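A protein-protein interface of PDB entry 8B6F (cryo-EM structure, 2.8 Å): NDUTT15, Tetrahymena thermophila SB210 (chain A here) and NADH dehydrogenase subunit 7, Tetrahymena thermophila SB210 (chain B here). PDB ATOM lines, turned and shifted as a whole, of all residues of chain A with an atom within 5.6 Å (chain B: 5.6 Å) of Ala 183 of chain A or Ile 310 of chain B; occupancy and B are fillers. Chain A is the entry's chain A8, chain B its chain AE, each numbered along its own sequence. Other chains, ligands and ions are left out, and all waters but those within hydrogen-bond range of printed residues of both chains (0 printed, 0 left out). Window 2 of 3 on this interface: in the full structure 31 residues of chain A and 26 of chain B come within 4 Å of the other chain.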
ATOM      1  N   HIS A 142     -22.048 -19.762 -16.186  1.00  0.00           N
ATOM      2  CA  HIS A 142     -20.685 -20.221 -16.431  1.00  0.00           C
ATOM      3  C   HIS A 142     -20.362 -20.216 -17.919  1.00  0.00           C
ATOM      4  O   HIS A 142     -19.267 -19.808 -18.322  1.00  0.00           O
ATOM      5  CB  HIS A 142     -20.485 -21.620 -15.852  1.00  0.00           C
ATOM      6  CG  HIS A 142     -19.099 -22.153 -16.040  1.00  0.00           C
ATOM      7  ND1 HIS A 142     -18.058 -21.831 -15.197  1.00  0.00           N
ATOM      8  CD2 HIS A 142     -18.578 -22.973 -16.984  1.00  0.00           C
ATOM      9  CE1 HIS A 142     -16.958 -22.435 -15.607  1.00  0.00           C
ATOM     10  NE2 HIS A 142     -17.246 -23.134 -16.691  1.00  0.00           N
ATOM     11  N   ALA A 145     -19.895 -16.679 -19.106  1.00  0.00           N
ATOM     12  CA  ALA A 145     -18.607 -16.207 -18.611  1.00  0.00           C
ATOM     13  C   ALA A 145     -17.464 -16.760 -19.451  1.00  0.00           C
ATOM     14  O   ALA A 145     -16.508 -16.041 -19.764  1.00  0.00           O
ATOM     15  CB  ALA A 145     -18.434 -16.598 -17.143  1.00  0.00           C
ATOM     16  N   THR A 146     -17.543 -18.038 -19.825  1.00  0.00           N
ATOM     17  CA  THR A 146     -16.519 -18.619 -20.688  1.00  0.00           C
ATOM     18  C   THR A 146     -16.464 -17.895 -22.026  1.00  0.00           C
ATOM     19  O   THR A 146     -15.378 -17.586 -22.529  1.00  0.00           O
ATOM     20  CB  THR A 146     -16.795 -20.109 -20.897  1.00  0.00           C
ATOM     21  OG1 THR A 146     -16.695 -20.796 -19.642  1.00  0.00           O
ATOM     22  CG2 THR A 146     -15.801 -20.718 -21.878  1.00  0.00           C
ATOM     23  N   LYS A 178     -18.513 -20.947  -8.292  1.00  0.00           N
ATOM     24  CA  LYS A 178     -17.338 -20.296  -7.725  1.00  0.00           C
ATOM     25  C   LYS A 178     -16.284 -20.053  -8.794  1.00  0.00           C
ATOM     26  O   LYS A 178     -15.671 -18.980  -8.841  1.00  0.00           O
ATOM     27  CB  LYS A 178     -16.771 -21.139  -6.584  1.00  0.00           C
ATOM     28  CG  LYS A 178     -15.638 -20.468  -5.829  1.00  0.00           C
ATOM     29  CD  LYS A 178     -15.229 -21.286  -4.616  1.00  0.00           C
ATOM     30  CE  LYS A 178     -14.140 -20.583  -3.819  1.00  0.00           C
ATOM     31  NZ  LYS A 178     -13.763 -21.349  -2.599  1.00  0.00           N
ATOM     32  N   ASP A 179     -16.053 -21.041  -9.660  1.00  0.00           N
ATOM     33  CA  ASP A 179     -15.095 -20.863 -10.745  1.00  0.00           C
ATOM     34  C   ASP A 179     -15.523 -19.730 -11.669  1.00  0.00           C
ATOM     35  O   ASP A 179     -14.707 -18.887 -12.058  1.00  0.00           O
ATOM     36  CB  ASP A 179     -14.948 -22.166 -11.529  1.00  0.00           C
ATOM     37  CG  ASP A 179     -14.045 -22.020 -12.736  1.00  0.00           C
ATOM     38  OD1 ASP A 179     -13.223 -21.081 -12.758  1.00  0.00           O
ATOM     39  OD2 ASP A 179     -14.165 -22.837 -13.668  1.00  0.00           O
ATOM     40  N   CYS A 180     -16.805 -19.699 -12.037  1.00  0.00           N
ATOM     41  CA  CYS A 180     -17.286 -18.659 -12.941  1.00  0.00           C
ATOM     42  C   CYS A 180     -17.089 -17.274 -12.338  1.00  0.00           C
ATOM     43  O   CYS A 180     -16.568 -16.366 -12.993  1.00  0.00           O
ATOM     44  CB  CYS A 180     -18.761 -18.898 -13.264  1.00  0.00           C
ATOM     45  SG  CYS A 180     -19.583 -17.496 -14.046  1.00  0.00           S
ATOM     46  N   PHE A 181     -17.504 -17.095 -11.083  1.00  0.00           N
ATOM     47  CA  PHE A 181     -17.428 -15.775 -10.465  1.00  0.00           C
ATOM     48  C   PHE A 181     -15.985 -15.358 -10.209  1.00  0.00           C
ATOM     49  O   PHE A 181     -15.640 -14.180 -10.358  1.00  0.00           O
ATOM     50  CB  PHE A 181     -18.242 -15.757  -9.174  1.00  0.00           C
ATOM     51  CG  PHE A 181     -19.704 -15.505  -9.395  1.00  0.00           C
ATOM     52  CD1 PHE A 181     -20.525 -16.499  -9.898  1.00  0.00           C
ATOM     53  CD2 PHE A 181     -20.253 -14.268  -9.112  1.00  0.00           C
ATOM     54  CE1 PHE A 181     -21.870 -16.265 -10.109  1.00  0.00           C
ATOM     55  CE2 PHE A 181     -21.598 -14.027  -9.322  1.00  0.00           C
ATOM     56  CZ  PHE A 181     -22.407 -15.028  -9.821  1.00  0.00           C
ATOM     57  N   THR A 182     -15.128 -16.303  -9.822  1.00  0.00           N
ATOM     58  CA  THR A 182     -13.718 -15.977  -9.636  1.00  0.00           C
ATOM     59  C   THR A 182     -13.072 -15.561 -10.950  1.00  0.00           C
ATOM     60  O   THR A 182     -12.303 -14.594 -10.994  1.00  0.00           O
ATOM     61  CB  THR A 182     -12.976 -17.171  -9.033  1.00  0.00           C
ATOM     62  OG1 THR A 182     -13.560 -17.517  -7.770  1.00  0.00           O
ATOM     63  CG2 THR A 182     -11.499 -16.846  -8.830  1.00  0.00           C
ATOM     64  N   ALA A 183     -13.375 -16.275 -12.034  1.00  0.00           N
ATOM     65  CA  ALA A 183     -12.820 -15.910 -13.332  1.00  0.00           C
ATOM     66  C   ALA A 183     -13.297 -14.532 -13.766  1.00  0.00           C
ATOM     67  O   ALA A 183     -12.511 -13.725 -14.276  1.00  0.00           O
ATOM     68  CB  ALA A 183     -13.197 -16.961 -14.375  1.00  0.00           C
ATOM     69  N   ARG A 184     -14.585 -14.244 -13.575  1.00  0.00           N
ATOM     70  CA  ARG A 184     -15.127 -12.951 -13.970  1.00  0.00           C
ATOM     71  C   ARG A 184     -14.695 -11.831 -13.036  1.00  0.00           C
ATOM     72  O   ARG A 184     -14.816 -10.658 -13.405  1.00  0.00           O
ATOM     73  CB  ARG A 184     -16.655 -13.015 -14.020  1.00  0.00           C
ATOM     74  CG  ARG A 184     -17.205 -13.903 -15.125  1.00  0.00           C
ATOM     75  CD  ARG A 184     -16.994 -13.285 -16.499  1.00  0.00           C
ATOM     76  NE  ARG A 184     -17.697 -12.017 -16.641  1.00  0.00           N
ATOM     77  CZ  ARG A 184     -17.635 -11.241 -17.715  1.00  0.00           C
ATOM     78  NH1 ARG A 184     -16.901 -11.570 -18.765  1.00  0.00           N
ATOM     79  NH2 ARG A 184     -18.326 -10.106 -17.735  1.00  0.00           N
ATOM     80  N   LYS A 185     -14.210 -12.160 -11.840  1.00  0.00           N
ATOM     81  CA  LYS A 185     -13.838 -11.219 -10.788  1.00  0.00           C
ATOM     82  C   LYS A 185     -15.054 -10.588 -10.124  1.00  0.00           C
ATOM     83  O   LYS A 185     -14.890  -9.819  -9.170  1.00  0.00           O
ATOM     84  CB  LYS A 185     -12.915 -10.102 -11.295  1.00  0.00           C
ATOM     85  CG  LYS A 185     -11.599 -10.611 -11.865  1.00  0.00           C
ATOM     86  CD  LYS A 185     -10.705  -9.461 -12.298  1.00  0.00           C
ATOM     87  CE  LYS A 185      -9.343  -9.957 -12.749  1.00  0.00           C
ATOM     88  NZ  LYS A 185      -8.602 -10.641 -11.652  1.00  0.00           N
ATOM     89  N   VAL B 308     -15.464 -26.868 -18.945  1.00  0.00           N
ATOM     90  CA  VAL B 308     -14.049 -26.546 -18.799  1.00  0.00           C
ATOM     91  C   VAL B 308     -13.937 -25.262 -17.993  1.00  0.00           C
ATOM     92  O   VAL B 308     -14.576 -24.257 -18.323  1.00  0.00           O
ATOM     93  CB  VAL B 308     -13.356 -26.396 -20.166  1.00  0.00           C
ATOM     94  CG1 VAL B 308     -11.899 -25.999 -19.992  1.00  0.00           C
ATOM     95  CG2 VAL B 308     -13.465 -27.687 -20.959  1.00  0.00           C
ATOM     96  N   SER B 309     -13.124 -25.297 -16.941  1.00  0.00           N
ATOM     97  CA  SER B 309     -12.940 -24.129 -16.093  1.00  0.00           C
ATOM     98  C   SER B 309     -12.261 -23.005 -16.865  1.00  0.00           C
ATOM     99  O   SER B 309     -11.331 -23.233 -17.642  1.00  0.00           O
ATOM    100  CB  SER B 309     -12.113 -24.492 -14.861  1.00  0.00           C
ATOM    101  OG  SER B 309     -10.867 -25.050 -15.230  1.00  0.00           O
ATOM    102  N   ILE B 310     -12.735 -21.778 -16.641  1.00  0.00           N
ATOM    103  CA  ILE B 310     -12.156 -20.624 -17.321  1.00  0.00           C
ATOM    104  C   ILE B 310     -10.745 -20.360 -16.815  1.00  0.00           C
ATOM    105  O   ILE B 310      -9.839 -20.044 -17.595  1.00  0.00           O
ATOM    106  CB  ILE B 310     -13.062 -19.390 -17.143  1.00  0.00           C
ATOM    107  CG1 ILE B 310     -14.475 -19.689 -17.653  1.00  0.00           C
ATOM    108  CG2 ILE B 310     -12.475 -18.192 -17.881  1.00  0.00           C
ATOM    109  CD1 ILE B 310     -15.484 -18.599 -17.353  1.00  0.00           C
ATOM    110  N   ASN B 311     -10.534 -20.477 -15.502  1.00  0.00           N
ATOM    111  CA  ASN B 311      -9.230 -20.157 -14.930  1.00  0.00           C
ATOM    112  C   ASN B 311      -8.182 -21.196 -15.312  1.00  0.00           C
ATOM    113  O   ASN B 311      -7.072 -20.847 -15.729  1.00  0.00           O
ATOM    114  CB  ASN B 311      -9.346 -20.052 -13.408  1.00  0.00           C
ATOM    115  CG  ASN B 311     -10.328 -18.986 -12.970  1.00  0.00           C
ATOM    116  OD1 ASN B 311     -10.458 -17.945 -13.613  1.00  0.00           O
ATOM    117  ND2 ASN B 311     -11.028 -19.241 -11.872  1.00  0.00           N
ATOM    118  N   THR B 312      -8.517 -22.480 -15.181  1.00  0.00           N
ATOM    119  CA  THR B 312      -7.541 -23.549 -15.344  1.00  0.00           C
ATOM    120  C   THR B 312      -7.616 -24.239 -16.699  1.00  0.00           C
ATOM    121  O   THR B 312      -6.673 -24.948 -17.066  1.00  0.00           O
ATOM    122  CB  THR B 312      -7.722 -24.600 -14.240  1.00  0.00           C
ATOM    123  OG1 THR B 312      -7.891 -23.944 -12.976  1.00  0.00           O
ATOM    124  CG2 THR B 312      -6.511 -25.517 -14.162  1.00  0.00           C
ATOM    125  N   LYS B 313      -8.695 -24.046 -17.454  1.00  0.00           N
ATOM    126  CA  LYS B 313      -8.857 -24.691 -18.756  1.00  0.00           C
ATOM    127  C   LYS B 313      -8.772 -26.211 -18.627  1.00  0.00           C
ATOM    128  O   LYS B 313      -8.189 -26.894 -19.472  1.00  0.00           O
ATOM    129  CB  LYS B 313      -7.820 -24.175 -19.756  1.00  0.00           C
ATOM    130  CG  LYS B 313      -7.791 -22.658 -19.907  1.00  0.00           C
ATOM    131  CD  LYS B 313      -9.135 -22.088 -20.351  1.00  0.00           C
ATOM    132  CE  LYS B 313      -9.562 -22.611 -21.716  1.00  0.00           C
ATOM    133  NZ  LYS B 313      -8.558 -22.317 -22.777  1.00  0.00           N
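A ring nitrogen (NE2) of His 142 of chain A sits at hydrogen-bond distance from the backbone carbonyl oxygen of Val 308 of chain B, at 3.3 Å. ND2 of Asn 311 of chain B lies within hydrogen-bond range of OD1 of Asp 179 of chain A. OD2 of Asp 179 of chain A sits at hydrogen-bond distance from N of Ile 310 of chain B (3.5 Å).
Of the 6 printed residues of chain B, 4 touch a printed residue of chain A. Hydrophobic or aromatic side chains of chain B within 4 Å of the printed part of chain A: Ile 310. Among the printed residues, 9 pairs touch across the chains.
Among the printed residues, merely in contact across the chains: Ala 145 of chain A with Ile 310 of chain B, Thr 146 of chain A with Ile 310 of chain B, Asp 179 of chain A with Ser 309 of chain B, Thr 182 of chain A with Asn 311 of chain B, Ala 183 of chain A with Ile 310 of chain B and Ala 183 of chain A with Asn 311 of chain B.
The side-chain hydroxyl (OG) of Ser 309 of chain B lies close to the backbone NH (N) of Thr 312 of chain B, at 3.5 Å. OG1 of Thr 146 of chain A lies within hydrogen-bond range of O of His 142 of chain A, 3.1 Å away. OG of Ser 309 of chain B sits at hydrogen-bond distance from N of Lys 313 of chain B (3.3 Å). The backbone carbonyl oxygen (O) of Lys 178 of chain A lies within hydrogen-bond range of the side-chain hydroxyl (OG1) of Thr 182 of chain A, at 2.8 Å.
Lys 178 of chain A touches none of the printed residues of chain B. Printed residues of chain B within 4 Å of Asp 179 of chain A: Ser 309, Ile 310 and Asn 311. Of the printed residues of chain B, Thr 182 of chain A touches Asn 311 (3.9 Å). Ala 183 of chain A touches just these residues of chain B: Ile 310 (3.7 Å) and Asn 311 (3.0 Å). Printed residues of chain A within 4 Å of Val 308 of chain B: His 142 (3.3 Å). Of the printed residues of chain A, Ser 309 of chain B touches Asp 179 (2.9 Å). Ile 310 of chain B touches just these residues of chain A: Ala 145, Thr 146, Asp 179 and Ala 183. Printed residues of chain A within 4 Å of Asn 311 of chain B: Asp 179, Thr 182 and Ala 183. The nearest printed residue of chain B that does not touch Ala 183 of chain A is Ser 309 of chain B (6.6 Å). The nearest residue of chain A that does not touch Ile 310 of chain B is His 142 of chain A (4.1 Å). The nearest printed residue of chain B that does not touch Asp 179 of chain A is Val 308 of chain B (4.9 Å).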
